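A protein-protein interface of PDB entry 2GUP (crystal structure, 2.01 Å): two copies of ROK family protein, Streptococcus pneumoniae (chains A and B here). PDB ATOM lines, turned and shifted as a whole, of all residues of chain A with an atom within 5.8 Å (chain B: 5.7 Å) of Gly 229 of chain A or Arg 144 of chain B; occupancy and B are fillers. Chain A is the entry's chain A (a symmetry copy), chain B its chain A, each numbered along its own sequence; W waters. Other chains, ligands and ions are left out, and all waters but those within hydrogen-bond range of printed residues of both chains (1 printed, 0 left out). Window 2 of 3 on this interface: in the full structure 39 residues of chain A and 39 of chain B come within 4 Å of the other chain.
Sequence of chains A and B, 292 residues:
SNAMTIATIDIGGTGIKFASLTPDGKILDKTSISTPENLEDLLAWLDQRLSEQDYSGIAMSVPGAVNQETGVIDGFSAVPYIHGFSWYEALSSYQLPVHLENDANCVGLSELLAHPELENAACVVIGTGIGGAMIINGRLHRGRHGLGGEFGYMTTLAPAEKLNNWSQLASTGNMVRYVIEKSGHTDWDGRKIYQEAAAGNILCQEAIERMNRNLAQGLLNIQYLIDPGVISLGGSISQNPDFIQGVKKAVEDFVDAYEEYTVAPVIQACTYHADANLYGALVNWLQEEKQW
OD2 of Asp 227 of chain A lies close to O of Gly 143 of chain B (3.3 Å). The side-chain carboxylate (OD2) of Asp 227 of chain A sits at hydrogen-bond distance from the backbone NH (N) of Arg 144 of chain B (3.2 Å). N of His 145 of chain B sits at hydrogen-bond distance from OD2 of Asp 227 of chain A, at 2.6 Å. The backbone NH (N) of Leu 147 of chain B sits at hydrogen-bond distance from the side-chain carboxylate (OD2) of Asp 227 of chain A (3.1 Å).
The backbone carbonyl oxygen of Pro 228 of chain A sits at hydrogen-bond distance from the side-chain amide nitrogen of Gln 223 of chain A. The side-chain carboxylate (OD1) of Asp 227 of chain A lies within hydrogen-bond range of the side-chain amide nitrogen (NE2) of Gln 223 of chain A (3.0 Å). O of Asn 120 of chain A lies within hydrogen-bond range of N of Gly 229 of chain A. The backbone carbonyl oxygen (O) of Arg 142 of chain B lies within hydrogen-bond range of the backbone NH (N) of Leu 147 of chain B.
His 145 of chain B touches Gln 223 of chain A (CE1 to NE2, 3.8 Å). Arg 142 of chain B touches Asp 227 of chain A (O to OD2, 3.8 Å). OD2 of Asp 227 of chain A touches N of Gly 146 of chain B, 3.5 Å away. CB of Arg 144 of chain B touches O of Pro 228 of chain A, at 3.97 Å. Gly 229 of chain A touches Arg 144 of chain B.
Asn 120 of chain A touches none of the printed residues of chain B. Ala 121 of chain A touches none of the printed residues of chain B. Printed residues of chain B within 4 Å of Asp 227 of chain A: Arg 142, Gly 143, Arg 144, His 145, Gly 146 and Leu 147. Printed residues of chain B within 4 Å of Pro 228 of chain A: Arg 144 (3.97 Å). Gly 229 of chain A touches one residue of chain B. Printed residues of chain A within 4 Å of Gly 143 of chain B: Asp 227. Of chain A, only Asp 227, Pro 228 and Gly 229 come within 4 Å of Arg 144 of chain B. Printed residues of chain A within 4 Å of Gly 146 of chain B: Asp 227. Of the printed residues of chain A, Leu 147 of chain B touches Asp 227 (3.1 Å). The nearest residue of chain A that does not touch Arg 144 of chain B is Asn 120 of chain A (4.1 Å).
Printed residues of chain B that touch a printed residue of chain A: Arg 142, Gly 143, Arg 144, His 145, Gly 146 and Leu 147. Hydrophobic or aromatic side chains of chain B that line the printed part of chain A: His 145 and Leu 147. Along chain A the printed residues that touch a printed residue of chain B span positions 223 to 229.
No position is printed for both chains. Of the 9 pairs that touch across the chains among the printed residues, none has its exchanged pair printed and touching as well.
Water W1 lies within hydrogen-bond range of the guanidinium group (NH1) of Arg 144 of chain B (2.8 Å) and the backbone NH (N) of Asn 120 of chain A (3.4 Å).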
ATOM      1  N   LEU A 118      -5.321  11.043 -17.105  1.00  0.00           N
ATOM      2  CA  LEU A 118      -4.974   9.641 -17.299  1.00  0.00           C
ATOM      3  C   LEU A 118      -5.745   9.160 -18.496  1.00  0.00           C
ATOM      4  O   LEU A 118      -6.943   9.407 -18.591  1.00  0.00           O
ATOM      5  CB  LEU A 118      -5.358   8.790 -16.074  1.00  0.00           C
ATOM      6  CG  LEU A 118      -4.273   8.715 -15.019  1.00  0.00           C
ATOM      7  CD1 LEU A 118      -4.763   8.299 -13.650  1.00  0.00           C
ATOM      8  CD2 LEU A 118      -3.202   7.747 -15.564  1.00  0.00           C
ATOM      9  N   ASN A 120      -4.391   5.681 -20.091  1.00  0.00           N
ATOM     10  CA  ASN A 120      -4.269   4.277 -19.788  1.00  0.00           C
ATOM     11  C   ASN A 120      -3.611   4.061 -18.431  1.00  0.00           C
ATOM     12  O   ASN A 120      -2.495   4.484 -18.226  1.00  0.00           O
ATOM     13  CB  ASN A 120      -3.454   3.523 -20.841  1.00  0.00           C
ATOM     14  CG  ASN A 120      -3.804   3.895 -22.272  1.00  0.00           C
ATOM     15  OD1 ASN A 120      -4.930   3.669 -22.793  1.00  0.00           O
ATOM     16  ND2 ASN A 120      -2.778   4.362 -22.967  1.00  0.00           N
ATOM     17  N   ALA A 121      -4.311   3.391 -17.539  1.00  0.00           N
ATOM     18  CA  ALA A 121      -3.928   3.218 -16.179  1.00  0.00           C
ATOM     19  C   ALA A 121      -4.371   1.873 -15.661  1.00  0.00           C
ATOM     20  O   ALA A 121      -5.317   1.336 -16.145  1.00  0.00           O
ATOM     21  CB  ALA A 121      -4.529   4.336 -15.352  1.00  0.00           C
ATOM     22  N   GLN A 223       2.526  -4.243 -16.535  1.00  0.00           N
ATOM     23  CA  GLN A 223       3.232  -3.293 -17.376  1.00  0.00           C
ATOM     24  C   GLN A 223       3.496  -3.873 -18.739  1.00  0.00           C
ATOM     25  O   GLN A 223       3.217  -3.205 -19.756  1.00  0.00           O
ATOM     26  CB  GLN A 223       4.588  -2.835 -16.768  1.00  0.00           C
ATOM     27  CG  GLN A 223       5.192  -1.615 -17.552  1.00  0.00           C
ATOM     28  CD  GLN A 223       4.236  -0.445 -17.469  1.00  0.00           C
ATOM     29  OE1 GLN A 223       3.710  -0.193 -16.386  1.00  0.00           O
ATOM     30  NE2 GLN A 223       3.915   0.199 -18.601  1.00  0.00           N
ATOM     31  N   ILE A 226      -0.382  -4.944 -20.480  1.00  0.00           N
ATOM     32  CA  ILE A 226      -1.352  -3.867 -20.942  1.00  0.00           C
ATOM     33  C   ILE A 226      -0.710  -2.515 -21.178  1.00  0.00           C
ATOM     34  O   ILE A 226      -1.347  -1.581 -21.753  1.00  0.00           O
ATOM     35  CB  ILE A 226      -2.577  -3.691 -19.993  1.00  0.00           C
ATOM     36  CG1 ILE A 226      -2.169  -3.170 -18.658  1.00  0.00           C
ATOM     37  CG2 ILE A 226      -3.285  -5.017 -19.774  1.00  0.00           C
ATOM     38  CD1 ILE A 226      -3.381  -2.647 -17.874  1.00  0.00           C
ATOM     39  N   ASP A 227       0.508  -2.393 -20.676  1.00  0.00           N
ATOM     40  CA  ASP A 227       1.364  -1.237 -20.841  1.00  0.00           C
ATOM     41  C   ASP A 227       0.605   0.096 -20.498  1.00  0.00           C
ATOM     42  O   ASP A 227       0.380   0.918 -21.377  1.00  0.00           O
ATOM     43  CB  ASP A 227       1.930  -1.217 -22.290  1.00  0.00           C
ATOM     44  CG  ASP A 227       2.952  -0.065 -22.522  1.00  0.00           C
ATOM     45  OD1 ASP A 227       3.726   0.274 -21.578  1.00  0.00           O
ATOM     46  OD2 ASP A 227       2.913   0.534 -23.630  1.00  0.00           O
ATOM     47  N   PRO A 228       0.224   0.279 -19.205  1.00  0.00           N
ATOM     48  CA  PRO A 228      -0.421   1.446 -18.715  1.00  0.00           C
ATOM     49  C   PRO A 228       0.599   2.635 -18.574  1.00  0.00           C
ATOM     50  O   PRO A 228       1.796   2.416 -18.478  1.00  0.00           O
ATOM     51  CB  PRO A 228      -0.987   0.968 -17.384  1.00  0.00           C
ATOM     52  CG  PRO A 228       0.105   0.002 -16.873  1.00  0.00           C
ATOM     53  CD  PRO A 228       0.455  -0.730 -18.105  1.00  0.00           C
ATOM     54  N   GLY A 229       0.131   3.895 -18.661  1.00  0.00           N
ATOM     55  CA  GLY A 229       1.001   5.036 -18.281  1.00  0.00           C
ATOM     56  C   GLY A 229       1.429   5.013 -16.807  1.00  0.00           C
ATOM     57  O   GLY A 229       2.559   5.398 -16.471  1.00  0.00           O
ATOM     58  N   VAL A 230       0.540   4.562 -15.924  1.00  0.00           N
ATOM     59  CA  VAL A 230       0.857   4.489 -14.486  1.00  0.00           C
ATOM     60  C   VAL A 230       0.158   3.281 -13.836  1.00  0.00           C
ATOM     61  O   VAL A 230      -0.872   2.855 -14.303  1.00  0.00           O
ATOM     62  CB  VAL A 230       0.459   5.832 -13.835  1.00  0.00           C
ATOM     63  CG1 VAL A 230      -1.094   6.070 -13.881  1.00  0.00           C
ATOM     64  CG2 VAL A 230       1.040   6.018 -12.390  1.00  0.00           C
ATOM     65  N   ILE A 231       0.759   2.658 -12.815  1.00  0.00           N
ATOM     66  CA  ILE A 231      -0.023   1.730 -11.990  1.00  0.00           C
ATOM     67  C   ILE A 231      -0.217   2.371 -10.575  1.00  0.00           C
ATOM     68  O   ILE A 231       0.770   2.738  -9.925  1.00  0.00           O
ATOM     69  CB  ILE A 231       0.639   0.421 -11.890  1.00  0.00           C
ATOM     70  CG1 ILE A 231       0.871  -0.146 -13.324  1.00  0.00           C
ATOM     71  CG2 ILE A 231      -0.269  -0.561 -11.057  1.00  0.00           C
ATOM     72  CD1 ILE A 231       1.975  -1.203 -13.480  1.00  0.00           C
ATOM     73  N   VAL A 266       5.682   3.062 -13.901  1.00  0.00           N
ATOM     74  CA  VAL A 266       5.486   4.103 -12.907  1.00  0.00           C
ATOM     75  C   VAL A 266       4.393   3.676 -11.907  1.00  0.00           C
ATOM     76  O   VAL A 266       3.243   3.400 -12.299  1.00  0.00           O
ATOM     77  CB  VAL A 266       5.434   5.618 -13.409  1.00  0.00           C
ATOM     78  CG1 VAL A 266       5.418   5.815 -14.937  1.00  0.00           C
ATOM     79  CG2 VAL A 266       4.478   6.558 -12.606  1.00  0.00           C
ATOM     80  N   ARG B 142      -2.283  -0.134 -28.237  1.00  0.00           N
ATOM     81  CA  ARG B 142      -0.805  -0.134 -28.321  1.00  0.00           C
ATOM     82  C   ARG B 142      -0.083   0.047 -26.961  1.00  0.00           C
ATOM     83  O   ARG B 142       1.011  -0.512 -26.752  1.00  0.00           O
ATOM     84  CB  ARG B 142      -0.305   0.888 -29.347  1.00  0.00           C
ATOM     85  CG  ARG B 142      -0.927   0.789 -30.779  1.00  0.00           C
ATOM     86  CD  ARG B 142       0.022   1.393 -31.842  1.00  0.00           C
ATOM     87  NE  ARG B 142      -0.475   1.224 -33.249  1.00  0.00           N
ATOM     88  CZ  ARG B 142      -1.606   1.748 -33.667  1.00  0.00           C
ATOM     89  NH1 ARG B 142      -2.336   2.429 -32.789  1.00  0.00           N
ATOM     90  NH2 ARG B 142      -2.017   1.555 -34.920  1.00  0.00           N
ATOM     91  N   GLY B 143      -0.666   0.853 -26.086  1.00  0.00           N
ATOM     92  CA  GLY B 143      -0.113   1.208 -24.764  1.00  0.00           C
ATOM     93  C   GLY B 143       0.892   2.366 -24.765  1.00  0.00           C
ATOM     94  O   GLY B 143       1.543   2.625 -25.769  1.00  0.00           O
ATOM     95  N   ARG B 144       1.026   3.071 -23.647  1.00  0.00           N
ATOM     96  CA  ARG B 144       2.065   4.143 -23.470  1.00  0.00           C
ATOM     97  C   ARG B 144       3.414   4.014 -24.239  1.00  0.00           C
ATOM     98  O   ARG B 144       3.938   4.981 -24.734  1.00  0.00           O
ATOM     99  CB  ARG B 144       2.384   4.262 -21.947  1.00  0.00           C
ATOM    100  CG  ARG B 144       3.175   5.513 -21.484  1.00  0.00           C
ATOM    101  CD  ARG B 144       2.357   6.759 -21.721  1.00  0.00           C
ATOM    102  NE  ARG B 144       2.881   7.894 -20.960  1.00  0.00           N
ATOM    103  CZ  ARG B 144       2.219   8.530 -19.977  1.00  0.00           C
ATOM    104  NH1 ARG B 144       0.969   8.179 -19.638  1.00  0.00           N
ATOM    105  NH2 ARG B 144       2.799   9.544 -19.330  1.00  0.00           N
ATOM    106  N   HIS B 145       3.995   2.829 -24.285  1.00  0.00           N
ATOM    107  CA  HIS B 145       5.333   2.575 -24.876  1.00  0.00           C
ATOM    108  C   HIS B 145       5.277   1.530 -26.001  1.00  0.00           C
ATOM    109  O   HIS B 145       6.236   0.751 -26.137  1.00  0.00           O
ATOM    110  CB  HIS B 145       6.279   1.932 -23.815  1.00  0.00           C
ATOM    111  CG  HIS B 145       6.271   2.626 -22.501  1.00  0.00           C
ATOM    112  ND1 HIS B 145       5.374   2.315 -21.501  1.00  0.00           N
ATOM    113  CD2 HIS B 145       7.024   3.649 -22.030  1.00  0.00           C
ATOM    114  CE1 HIS B 145       5.583   3.110 -20.463  1.00  0.00           C
ATOM    115  NE2 HIS B 145       6.583   3.922 -20.757  1.00  0.00           N
ATOM    116  N   GLY B 146       4.167   1.485 -26.760  1.00  0.00           N
ATOM    117  CA  GLY B 146       3.892   0.410 -27.714  1.00  0.00           C
ATOM    118  C   GLY B 146       4.211  -0.992 -27.175  1.00  0.00           C
ATOM    119  O   GLY B 146       4.686  -1.852 -27.919  1.00  0.00           O
ATOM    120  N   LEU B 147       3.947  -1.258 -25.912  1.00  0.00           N
ATOM    121  CA  LEU B 147       4.144  -2.619 -25.397  1.00  0.00           C
ATOM    122  C   LEU B 147       2.826  -3.390 -25.173  1.00  0.00           C
ATOM    123  O   LEU B 147       2.860  -4.487 -24.632  1.00  0.00           O
ATOM    124  CB  LEU B 147       5.046  -2.672 -24.130  1.00  0.00           C
ATOM    125  CG  LEU B 147       6.604  -2.534 -24.122  1.00  0.00           C
ATOM    126  CD1 LEU B 147       7.077  -2.070 -22.714  1.00  0.00           C
ATOM    127  CD2 LEU B 147       7.471  -3.900 -24.514  1.00  0.00           C
HETATM  128  O   HOH W   1      -1.734   7.672 -19.322  1.00  0.00           O
